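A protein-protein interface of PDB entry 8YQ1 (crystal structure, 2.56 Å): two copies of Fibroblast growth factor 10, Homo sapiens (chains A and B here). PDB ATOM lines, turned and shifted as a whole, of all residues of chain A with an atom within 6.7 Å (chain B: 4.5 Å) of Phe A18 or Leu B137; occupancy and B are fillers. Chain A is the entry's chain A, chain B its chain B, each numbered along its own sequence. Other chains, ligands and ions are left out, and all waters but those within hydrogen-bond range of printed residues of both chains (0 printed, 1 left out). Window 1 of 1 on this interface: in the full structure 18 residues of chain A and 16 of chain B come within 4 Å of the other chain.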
ATOM      1  N   LYS A  16       2.326 -19.589   4.027  1.00  0.00           N
ATOM      2  CA  LYS A  16       1.564 -20.579   3.266  1.00  0.00           C
ATOM      3  C   LYS A  16       1.921 -20.446   1.781  1.00  0.00           C
ATOM      4  O   LYS A  16       2.138 -19.338   1.283  1.00  0.00           O
ATOM      5  CB  LYS A  16       0.052 -20.375   3.460  1.00  0.00           C
ATOM      6  CG  LYS A  16      -0.526 -20.723   4.823  1.00  0.00           C
ATOM      7  CD  LYS A  16      -1.909 -20.141   5.024  1.00  0.00           C
ATOM      8  CE  LYS A  16      -2.511 -20.351   6.404  1.00  0.00           C
ATOM      9  NZ  LYS A  16      -3.374 -21.557   6.464  1.00  0.00           N
ATOM     10  N   LEU A  17       1.953 -21.568   1.056  1.00  0.00           N
ATOM     11  CA  LEU A  17       2.155 -21.513  -0.396  1.00  0.00           C
ATOM     12  C   LEU A  17       0.882 -21.917  -1.128  1.00  0.00           C
ATOM     13  O   LEU A  17       0.440 -23.049  -0.993  1.00  0.00           O
ATOM     14  CB  LEU A  17       3.307 -22.440  -0.804  1.00  0.00           C
ATOM     15  CG  LEU A  17       4.678 -21.947  -0.356  1.00  0.00           C
ATOM     16  CD1 LEU A  17       5.767 -22.927  -0.718  1.00  0.00           C
ATOM     17  CD2 LEU A  17       4.952 -20.572  -0.941  1.00  0.00           C
ATOM     18  N   PHE A  18       0.314 -20.993  -1.899  1.00  0.00           N
ATOM     19  CA  PHE A  18      -0.989 -21.190  -2.517  1.00  0.00           C
ATOM     20  C   PHE A  18      -0.806 -21.238  -4.028  1.00  0.00           C
ATOM     21  O   PHE A  18      -0.375 -20.250  -4.634  1.00  0.00           O
ATOM     22  CB  PHE A  18      -1.937 -20.059  -2.085  1.00  0.00           C
ATOM     23  CG  PHE A  18      -3.363 -20.149  -2.568  1.00  0.00           C
ATOM     24  CD1 PHE A  18      -4.241 -21.073  -2.014  1.00  0.00           C
ATOM     25  CD2 PHE A  18      -3.831 -19.300  -3.562  1.00  0.00           C
ATOM     26  CE1 PHE A  18      -5.553 -21.165  -2.455  1.00  0.00           C
ATOM     27  CE2 PHE A  18      -5.150 -19.381  -3.998  1.00  0.00           C
ATOM     28  CZ  PHE A  18      -6.008 -20.314  -3.440  1.00  0.00           C
ATOM     29  N   SER A  19      -1.112 -22.391  -4.632  1.00  0.00           N
ATOM     30  CA  SER A  19      -0.897 -22.541  -6.065  1.00  0.00           C
ATOM     31  C   SER A  19      -1.987 -21.800  -6.822  1.00  0.00           C
ATOM     32  O   SER A  19      -3.041 -21.498  -6.290  1.00  0.00           O
ATOM     33  CB  SER A  19      -0.798 -23.963  -6.491  1.00  0.00           C
ATOM     34  OG  SER A  19      -1.997 -24.650  -6.241  1.00  0.00           O
ATOM     35  N   PHE A  20      -1.668 -21.463  -8.056  1.00  0.00           N
ATOM     36  CA  PHE A  20      -2.595 -20.838  -8.976  1.00  0.00           C
ATOM     37  C   PHE A  20      -3.690 -21.849  -9.336  1.00  0.00           C
ATOM     38  O   PHE A  20      -4.741 -21.464  -9.844  1.00  0.00           O
ATOM     39  CB  PHE A  20      -1.824 -20.285 -10.190  1.00  0.00           C
ATOM     40  CG  PHE A  20      -1.082 -18.989  -9.944  1.00  0.00           C
ATOM     41  CD1 PHE A  20      -0.548 -18.676  -8.701  1.00  0.00           C
ATOM     42  CD2 PHE A  20      -0.881 -18.085 -10.971  1.00  0.00           C
ATOM     43  CE1 PHE A  20       0.117 -17.477  -8.483  1.00  0.00           C
ATOM     44  CE2 PHE A  20      -0.182 -16.906 -10.764  1.00  0.00           C
ATOM     45  CZ  PHE A  20       0.310 -16.593  -9.516  1.00  0.00           C
ATOM     46  N   THR A  21      -3.466 -23.134  -9.027  1.00  0.00           N
ATOM     47  CA  THR A  21      -4.530 -24.127  -9.080  1.00  0.00           C
ATOM     48  C   THR A  21      -5.442 -24.055  -7.860  1.00  0.00           C
ATOM     49  O   THR A  21      -6.376 -24.843  -7.770  1.00  0.00           O
ATOM     50  CB  THR A  21      -3.977 -25.541  -9.266  1.00  0.00           C
ATOM     51  OG1 THR A  21      -2.889 -25.783  -8.376  1.00  0.00           O
ATOM     52  CG2 THR A  21      -3.522 -25.738 -10.694  1.00  0.00           C
ATOM     53  N   LYS A  22      -5.189 -23.085  -6.969  1.00  0.00           N
ATOM     54  CA  LYS A  22      -6.063 -22.692  -5.864  1.00  0.00           C
ATOM     55  C   LYS A  22      -6.016 -23.700  -4.723  1.00  0.00           C
ATOM     56  O   LYS A  22      -6.992 -23.788  -3.981  1.00  0.00           O
ATOM     57  CB  LYS A  22      -7.535 -22.494  -6.249  1.00  0.00           C
ATOM     58  CG  LYS A  22      -7.803 -21.808  -7.576  1.00  0.00           C
ATOM     59  CD  LYS A  22      -7.218 -20.448  -7.689  1.00  0.00           C
ATOM     60  CE  LYS A  22      -7.913 -19.582  -8.720  1.00  0.00           C
ATOM     61  NZ  LYS A  22      -7.602 -19.967 -10.116  1.00  0.00           N
ATOM     62  N   TYR A  23      -4.859 -24.371  -4.522  1.00  0.00           N
ATOM     63  CA  TYR A  23      -4.626 -25.107  -3.279  1.00  0.00           C
ATOM     64  C   TYR A  23      -3.475 -24.519  -2.461  1.00  0.00           C
ATOM     65  O   TYR A  23      -2.498 -24.025  -2.999  1.00  0.00           O
ATOM     66  CB  TYR A  23      -4.334 -26.583  -3.508  1.00  0.00           C
ATOM     67  CG  TYR A  23      -5.434 -27.301  -4.266  1.00  0.00           C
ATOM     68  CD1 TYR A  23      -5.528 -27.189  -5.645  1.00  0.00           C
ATOM     69  CD2 TYR A  23      -6.407 -28.043  -3.595  1.00  0.00           C
ATOM     70  CE1 TYR A  23      -6.535 -27.824  -6.343  1.00  0.00           C
ATOM     71  CE2 TYR A  23      -7.425 -28.679  -4.283  1.00  0.00           C
ATOM     72  CZ  TYR A  23      -7.485 -28.562  -5.661  1.00  0.00           C
ATOM     73  OH  TYR A  23      -8.449 -29.197  -6.374  1.00  0.00           O
ATOM     74  N   PHE A  24      -3.641 -24.555  -1.132  1.00  0.00           N
ATOM     75  CA  PHE A  24      -2.546 -24.487  -0.178  1.00  0.00           C
ATOM     76  C   PHE A  24      -1.810 -25.826  -0.104  1.00  0.00           C
ATOM     77  O   PHE A  24      -2.421 -26.884   0.021  1.00  0.00           O
ATOM     78  CB  PHE A  24      -3.058 -24.169   1.228  1.00  0.00           C
ATOM     79  CG  PHE A  24      -3.693 -22.810   1.378  1.00  0.00           C
ATOM     80  CD1 PHE A  24      -2.912 -21.667   1.474  1.00  0.00           C
ATOM     81  CD2 PHE A  24      -5.071 -22.676   1.399  1.00  0.00           C
ATOM     82  CE1 PHE A  24      -3.497 -20.415   1.620  1.00  0.00           C
ATOM     83  CE2 PHE A  24      -5.651 -21.428   1.562  1.00  0.00           C
ATOM     84  CZ  PHE A  24      -4.866 -20.301   1.655  1.00  0.00           C
ATOM     85  N   LEU A  25      -0.479 -25.756  -0.166  1.00  0.00           N
ATOM     86  CA  LEU A  25       0.375 -26.924  -0.053  1.00  0.00           C
ATOM     87  C   LEU A  25       0.497 -27.344   1.412  1.00  0.00           C
ATOM     88  O   LEU A  25       0.692 -26.484   2.277  1.00  0.00           O
ATOM     89  CB  LEU A  25       1.742 -26.547  -0.625  1.00  0.00           C
ATOM     90  CG  LEU A  25       2.780 -27.656  -0.570  1.00  0.00           C
ATOM     91  CD1 LEU A  25       2.548 -28.623  -1.713  1.00  0.00           C
ATOM     92  CD2 LEU A  25       4.174 -27.070  -0.646  1.00  0.00           C
ATOM     93  N   THR A  36      -4.859 -28.371  -0.287  1.00  0.00           N
ATOM     94  CA  THR A  36      -6.128 -28.267   0.408  1.00  0.00           C
ATOM     95  C   THR A  36      -6.747 -26.916   0.097  1.00  0.00           C
ATOM     96  O   THR A  36      -6.038 -25.908  -0.011  1.00  0.00           O
ATOM     97  CB  THR A  36      -6.093 -28.064   1.934  1.00  0.00           C
ATOM     98  OG1 THR A  36      -4.794 -28.241   2.480  1.00  0.00           O
ATOM     99  CG2 THR A  36      -7.106 -28.919   2.661  1.00  0.00           C
ATOM    100  N   LYS A  37      -8.079 -26.908   0.130  1.00  0.00           N
ATOM    101  CA  LYS A  37      -8.830 -25.683  -0.005  1.00  0.00           C
ATOM    102  C   LYS A  37      -8.932 -25.011   1.353  1.00  0.00           C
ATOM    103  O   LYS A  37      -9.296 -23.841   1.433  1.00  0.00           O
ATOM    104  CB  LYS A  37     -10.196 -25.973  -0.623  1.00  0.00           C
ATOM    105  CG  LYS A  37     -10.386 -25.416  -2.024  1.00  0.00           C
ATOM    106  CD  LYS A  37      -9.853 -26.247  -3.156  1.00  0.00           C
ATOM    107  CE  LYS A  37      -9.728 -25.417  -4.417  1.00  0.00           C
ATOM    108  NZ  LYS A  37      -9.859 -26.227  -5.648  1.00  0.00           N
ATOM    109  N   GLU A  39      -8.244 -22.929   4.313  1.00  0.00           N
ATOM    110  CA  GLU A  39      -7.449 -21.774   4.731  1.00  0.00           C
ATOM    111  C   GLU A  39      -6.928 -21.878   6.168  1.00  0.00           C
ATOM    112  O   GLU A  39      -6.192 -21.004   6.612  1.00  0.00           O
ATOM    113  CB  GLU A  39      -8.282 -20.491   4.695  1.00  0.00           C
ATOM    114  CG  GLU A  39      -8.528 -19.950   3.304  1.00  0.00           C
ATOM    115  CD  GLU A  39      -9.243 -18.610   3.323  1.00  0.00           C
ATOM    116  OE1 GLU A  39     -10.410 -18.556   2.844  1.00  0.00           O
ATOM    117  OE2 GLU A  39      -8.630 -17.622   3.825  1.00  0.00           O
ATOM    118  N   LEU A 115       1.023 -28.348  -8.006  1.00  0.00           N
ATOM    119  CA  LEU A 115      -0.235 -28.956  -7.578  1.00  0.00           C
ATOM    120  C   LEU A 115      -1.218 -28.853  -8.724  1.00  0.00           C
ATOM    121  O   LEU A 115      -1.475 -27.747  -9.223  1.00  0.00           O
ATOM    122  CB  LEU A 115      -0.810 -28.280  -6.326  1.00  0.00           C
ATOM    123  CG  LEU A 115       0.100 -28.366  -5.104  1.00  0.00           C
ATOM    124  CD1 LEU A 115      -0.433 -27.567  -3.923  1.00  0.00           C
ATOM    125  CD2 LEU A 115       0.322 -29.812  -4.734  1.00  0.00           C
ATOM    126  N   HIS A 135       2.835 -22.397 -10.008  1.00  0.00           N
ATOM    127  CA  HIS A 135       2.943 -21.016  -9.585  1.00  0.00           C
ATOM    128  C   HIS A 135       2.396 -20.887  -8.165  1.00  0.00           C
ATOM    129  O   HIS A 135       1.390 -21.510  -7.835  1.00  0.00           O
ATOM    130  CB  HIS A 135       2.114 -20.119 -10.495  1.00  0.00           C
ATOM    131  CG  HIS A 135       2.665 -19.995 -11.861  1.00  0.00           C
ATOM    132  ND1 HIS A 135       3.806 -20.635 -12.262  1.00  0.00           N
ATOM    133  CD2 HIS A 135       2.232 -19.285 -12.918  1.00  0.00           C
ATOM    134  CE1 HIS A 135       4.041 -20.323 -13.535  1.00  0.00           C
ATOM    135  NE2 HIS A 135       3.098 -19.495 -13.948  1.00  0.00           N
ATOM    136  N   PHE A 136       3.066 -20.075  -7.337  1.00  0.00           N
ATOM    137  CA  PHE A 136       2.788 -20.052  -5.913  1.00  0.00           C
ATOM    138  C   PHE A 136       2.809 -18.619  -5.423  1.00  0.00           C
ATOM    139  O   PHE A 136       3.786 -17.908  -5.642  1.00  0.00           O
ATOM    140  CB  PHE A 136       3.787 -20.920  -5.154  1.00  0.00           C
ATOM    141  CG  PHE A 136       3.512 -22.394  -5.231  1.00  0.00           C
ATOM    142  CD1 PHE A 136       2.602 -22.993  -4.373  1.00  0.00           C
ATOM    143  CD2 PHE A 136       4.118 -23.177  -6.184  1.00  0.00           C
ATOM    144  CE1 PHE A 136       2.371 -24.358  -4.420  1.00  0.00           C
ATOM    145  CE2 PHE A 136       3.881 -24.545  -6.228  1.00  0.00           C
ATOM    146  CZ  PHE A 136       3.000 -25.130  -5.355  1.00  0.00           C
ATOM    147  N   LEU A 137       1.680 -18.217  -4.825  1.00  0.00           N
ATOM    148  CA  LEU A 137       1.559 -16.944  -4.138  1.00  0.00           C
ATOM    149  C   LEU A 137       1.808 -17.200  -2.651  1.00  0.00           C
ATOM    150  O   LEU A 137       0.970 -17.767  -1.956  1.00  0.00           O
ATOM    151  CB  LEU A 137       0.172 -16.362  -4.420  1.00  0.00           C
ATOM    152  CG  LEU A 137      -0.053 -14.925  -3.955  1.00  0.00           C
ATOM    153  CD1 LEU A 137      -0.127 -14.859  -2.447  1.00  0.00           C
ATOM    154  CD2 LEU A 137       1.057 -13.995  -4.430  1.00  0.00           C
ATOM    155  N   PRO A 138       2.997 -16.839  -2.120  1.00  0.00           N
ATOM    156  CA  PRO A 138       3.283 -17.027  -0.707  1.00  0.00           C
ATOM    157  C   PRO A 138       2.522 -15.980   0.095  1.00  0.00           C
ATOM    158  O   PRO A 138       2.393 -14.838  -0.326  1.00  0.00           O
ATOM    159  CB  PRO A 138       4.811 -16.897  -0.654  1.00  0.00           C
ATOM    160  CG  PRO A 138       5.141 -15.939  -1.753  1.00  0.00           C
ATOM    161  CD  PRO A 138       4.126 -16.227  -2.830  1.00  0.00           C
ATOM    162  N   MET A 139       1.990 -16.409   1.234  1.00  0.00           N
ATOM    163  CA  MET A 139       1.146 -15.590   2.082  1.00  0.00           C
ATOM    164  C   MET A 139       1.724 -15.658   3.485  1.00  0.00           C
ATOM    165  O   MET A 139       2.069 -16.742   3.941  1.00  0.00           O
ATOM    166  CB  MET A 139      -0.288 -16.133   2.073  1.00  0.00           C
ATOM    167  CG  MET A 139      -1.079 -15.799   0.787  1.00  0.00           C
ATOM    168  SD  MET A 139      -2.638 -16.742   0.690  1.00  0.00           S
ATOM    169  CE  MET A 139      -3.449 -16.097   2.153  1.00  0.00           C
ATOM    170  N   LYS B  16     -13.104 -15.770  -1.703  1.00  0.00           N
ATOM    171  CA  LYS B  16     -12.469 -14.491  -1.445  1.00  0.00           C
ATOM    172  C   LYS B  16     -11.691 -14.115  -2.698  1.00  0.00           C
ATOM    173  O   LYS B  16     -11.331 -14.986  -3.475  1.00  0.00           O
ATOM    174  CB  LYS B  16     -11.554 -14.577  -0.219  1.00  0.00           C
ATOM    175  CG  LYS B  16     -12.265 -14.690   1.129  1.00  0.00           C
ATOM    176  CD  LYS B  16     -11.493 -15.491   2.168  1.00  0.00           C
ATOM    177  CE  LYS B  16     -12.256 -15.768   3.446  1.00  0.00           C
ATOM    178  NZ  LYS B  16     -11.720 -15.017   4.610  1.00  0.00           N
ATOM    179  N   LEU B  17     -11.417 -12.822  -2.867  1.00  0.00           N
ATOM    180  CA  LEU B  17     -10.515 -12.334  -3.902  1.00  0.00           C
ATOM    181  C   LEU B  17      -9.302 -11.711  -3.222  1.00  0.00           C
ATOM    182  O   LEU B  17      -9.419 -10.734  -2.477  1.00  0.00           O
ATOM    183  CB  LEU B  17     -11.231 -11.311  -4.802  1.00  0.00           C
ATOM    184  CG  LEU B  17     -12.302 -11.903  -5.722  1.00  0.00           C
ATOM    185  CD1 LEU B  17     -13.037 -10.833  -6.505  1.00  0.00           C
ATOM    186  CD2 LEU B  17     -11.702 -12.900  -6.681  1.00  0.00           C
ATOM    187  N   PHE B  18      -8.142 -12.294  -3.526  1.00  0.00           N
ATOM    188  CA  PHE B  18      -6.886 -11.936  -2.907  1.00  0.00           C
ATOM    189  C   PHE B  18      -6.050 -11.163  -3.909  1.00  0.00           C
ATOM    190  O   PHE B  18      -5.650 -11.744  -4.920  1.00  0.00           O
ATOM    191  CB  PHE B  18      -6.122 -13.188  -2.475  1.00  0.00           C
ATOM    192  CG  PHE B  18      -4.991 -12.914  -1.512  1.00  0.00           C
ATOM    193  CD1 PHE B  18      -5.260 -12.469  -0.225  1.00  0.00           C
ATOM    194  CD2 PHE B  18      -3.669 -13.092  -1.890  1.00  0.00           C
ATOM    195  CE1 PHE B  18      -4.231 -12.227   0.669  1.00  0.00           C
ATOM    196  CE2 PHE B  18      -2.644 -12.824  -0.998  1.00  0.00           C
ATOM    197  CZ  PHE B  18      -2.925 -12.391   0.278  1.00  0.00           C
ATOM    198  N   PHE B  20      -2.722  -9.215  -5.460  1.00  0.00           N
ATOM    199  CA  PHE B  20      -1.297  -9.488  -5.426  1.00  0.00           C
ATOM    200  C   PHE B  20      -0.578  -8.459  -4.552  1.00  0.00           C
ATOM    201  O   PHE B  20       0.552  -8.707  -4.138  1.00  0.00           O
ATOM    202  CB  PHE B  20      -0.737  -9.615  -6.848  1.00  0.00           C
ATOM    203  CG  PHE B  20      -0.866 -11.028  -7.351  1.00  0.00           C
ATOM    204  CD1 PHE B  20      -2.115 -11.588  -7.569  1.00  0.00           C
ATOM    205  CD2 PHE B  20       0.247 -11.830  -7.528  1.00  0.00           C
ATOM    206  CE1 PHE B  20      -2.246 -12.905  -7.991  1.00  0.00           C
ATOM    207  CE2 PHE B  20       0.117 -13.142  -7.964  1.00  0.00           C
ATOM    208  CZ  PHE B  20      -1.130 -13.680  -8.187  1.00  0.00           C
ATOM    209  N   GLY B  95      -1.659 -16.475 -14.879  1.00  0.00           N
ATOM    210  CA  GLY B  95      -2.672 -17.307 -14.252  1.00  0.00           C
ATOM    211  C   GLY B  95      -3.451 -16.583 -13.149  1.00  0.00           C
ATOM    212  O   GLY B  95      -4.230 -17.197 -12.444  1.00  0.00           O
ATOM    213  N   TYR B  96      -3.272 -15.282 -12.971  1.00  0.00           N
ATOM    214  CA  TYR B  96      -4.138 -14.570 -12.044  1.00  0.00           C
ATOM    215  C   TYR B  96      -5.272 -13.908 -12.829  1.00  0.00           C
ATOM    216  O   TYR B  96      -5.305 -13.946 -14.051  1.00  0.00           O
ATOM    217  CB  TYR B  96      -3.347 -13.596 -11.163  1.00  0.00           C
ATOM    218  CG  TYR B  96      -2.276 -12.893 -11.966  1.00  0.00           C
ATOM    219  CD1 TYR B  96      -2.608 -11.947 -12.928  1.00  0.00           C
ATOM    220  CD2 TYR B  96      -0.945 -13.257 -11.811  1.00  0.00           C
ATOM    221  CE1 TYR B  96      -1.627 -11.347 -13.697  1.00  0.00           C
ATOM    222  CE2 TYR B  96       0.035 -12.673 -12.582  1.00  0.00           C
ATOM    223  CZ  TYR B  96      -0.308 -11.730 -13.532  1.00  0.00           C
ATOM    224  OH  TYR B  96       0.697 -11.183 -14.263  1.00  0.00           O
ATOM    225  N   PHE B 136      -5.851 -10.641  -9.054  1.00  0.00           N
ATOM    226  CA  PHE B 136      -6.443 -11.384  -7.949  1.00  0.00           C
ATOM    227  C   PHE B 136      -6.355 -12.890  -8.198  1.00  0.00           C
ATOM    228  O   PHE B 136      -6.366 -13.367  -9.336  1.00  0.00           O
ATOM    229  CB  PHE B 136      -7.900 -10.970  -7.724  1.00  0.00           C
ATOM    230  CG  PHE B 136      -8.102  -9.521  -7.355  1.00  0.00           C
ATOM    231  CD1 PHE B 136      -8.013  -8.520  -8.317  1.00  0.00           C
ATOM    232  CD2 PHE B 136      -8.337  -9.146  -6.031  1.00  0.00           C
ATOM    233  CE1 PHE B 136      -8.180  -7.186  -7.977  1.00  0.00           C
ATOM    234  CE2 PHE B 136      -8.474  -7.807  -5.688  1.00  0.00           C
ATOM    235  CZ  PHE B 136      -8.395  -6.831  -6.659  1.00  0.00           C
ATOM    236  N   LEU B 137      -6.276 -13.638  -7.100  1.00  0.00           N
ATOM    237  CA  LEU B 137      -6.601 -15.048  -7.076  1.00  0.00           C
ATOM    238  C   LEU B 137      -7.906 -15.221  -6.307  1.00  0.00           C
ATOM    239  O   LEU B 137      -7.996 -14.832  -5.154  1.00  0.00           O
ATOM    240  CB  LEU B 137      -5.468 -15.795  -6.352  1.00  0.00           C
ATOM    241  CG  LEU B 137      -4.247 -16.266  -7.150  1.00  0.00           C
ATOM    242  CD1 LEU B 137      -3.809 -17.609  -6.643  1.00  0.00           C
ATOM    243  CD2 LEU B 137      -4.506 -16.365  -8.640  1.00  0.00           C
ATOM    244  N   PRO B 138      -8.966 -15.842  -6.850  1.00  0.00           N
ATOM    245  CA  PRO B 138     -10.110 -16.224  -6.012  1.00  0.00           C
ATOM    246  C   PRO B 138      -9.703 -17.414  -5.155  1.00  0.00           C
ATOM    247  O   PRO B 138      -8.945 -18.252  -5.641  1.00  0.00           O
ATOM    248  CB  PRO B 138     -11.216 -16.595  -7.005  1.00  0.00           C
ATOM    249  CG  PRO B 138     -10.472 -16.941  -8.311  1.00  0.00           C
ATOM    250  CD  PRO B 138      -9.150 -16.191  -8.266  1.00  0.00           C
ATOM    251  N   MET B 139     -10.109 -17.442  -3.876  1.00  0.00           N
ATOM    252  CA  MET B 139      -9.896 -18.629  -3.050  1.00  0.00           C
ATOM    253  C   MET B 139     -11.251 -19.153  -2.594  1.00  0.00           C
ATOM    254  O   MET B 139     -12.150 -18.380  -2.287  1.00  0.00           O
ATOM    255  CB  MET B 139      -9.004 -18.388  -1.826  1.00  0.00           C
ATOM    256  CG  MET B 139      -8.184 -17.098  -1.866  1.00  0.00           C
ATOM    257  SD  MET B 139      -6.895 -16.969  -0.544  1.00  0.00           S
ATOM    258  CE  MET B 139      -5.453 -17.525  -1.448  1.00  0.00           C
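Of the 19 printed residues of chain A, 7 touch a printed residue of chain B. Hydrophobic or aromatic side chains of chain A within 4 Å of the printed part of chain B: Phe A18, Phe A20, Leu A137 and Met A139. Hydrophobic or aromatic side chains of chain B within 4 Å of the printed part of chain A: Phe B18, Phe B20, Tyr B96, Leu B137, Pro B138 and Met B139. Among the printed residues, 12 pairs touch across the chains. Among the printed residues, no Asp or Glu carboxylate lies within 4 Å of a Lys or Arg side-chain nitrogen of the other chain.
Among the printed residues, pairs that only touch across the chains: Phe A18 with Met B139 (3.2 Å), Glu A39 with Lys B16 (3.3 Å), Phe A18 with Leu B137 (3.5 Å), Lys A22 with Pro B138 (3.5 Å), Phe A20 with Phe B20 (3.5 Å), Leu A137 with Phe B18 (3.5 Å), Met A139 with Met B139 (3.6 Å), Phe A20 with Gly B95 (3.7 Å), Leu A137 with Phe B20 (3.8 Å), Met A139 with Phe B18 (3.8 Å), Phe A20 with Tyr B96 (3.9 Å) and Ser A19 with Leu B137 (3.98 Å).
Of the printed residues of chain B, Phe A18 touches Leu B137 and Met B139. Printed residues of chain B within 4 Å of Ser A19: Leu B137 (3.98 Å). Lys A37 touches none of the printed residues of chain B. Of the printed residues of chain A, Tyr B96 touches Phe A20 (3.9 Å). Of the printed residues of chain A, Leu B137 touches Phe A18 and Ser A19. Printed residues of chain A within 4 Å of Pro B138: Lys A22 (3.5 Å). The nearest printed residue of chain B that does not touch Ser A19 is Met B139 (6.7 Å).
Phe A18 touches Leu B137, and with the chains exchanged Leu A137 touches Phe B18. Phe B20 touches its own counterpart, Phe A20. Leu A137 touches Phe B20, but with the chains exchanged Phe A20 does not touch Leu B137 (4.001 Å). Met B139 touches its own counterpart, Met A139. 8 positions are printed for both chains. Of the 12 pairs that touch across the chains among the printed residues, 6 have their exchanged pair printed and touching as well.
O of Phe A20 sits at hydrogen-bond distance from NZ of Lys A22, at 3.2 Å. The backbone carbonyl oxygen (O) of Lys B16 sits at hydrogen-bond distance from the backbone NH (N) of Met B139. N of Phe A20 sits at hydrogen-bond distance from O of His A135 (3.1 Å). The side-chain hydroxyl (OG) of Ser A19 sits at hydrogen-bond distance from the backbone carbonyl oxygen (O) of Tyr A23. The backbone carbonyl oxygen (O) of Phe A18 lies within hydrogen-bond range of the backbone NH (N) of Leu A137, 2.9 Å away. N of Leu B137 lies within hydrogen-bond range of O of Phe B18, 3.0 Å away.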
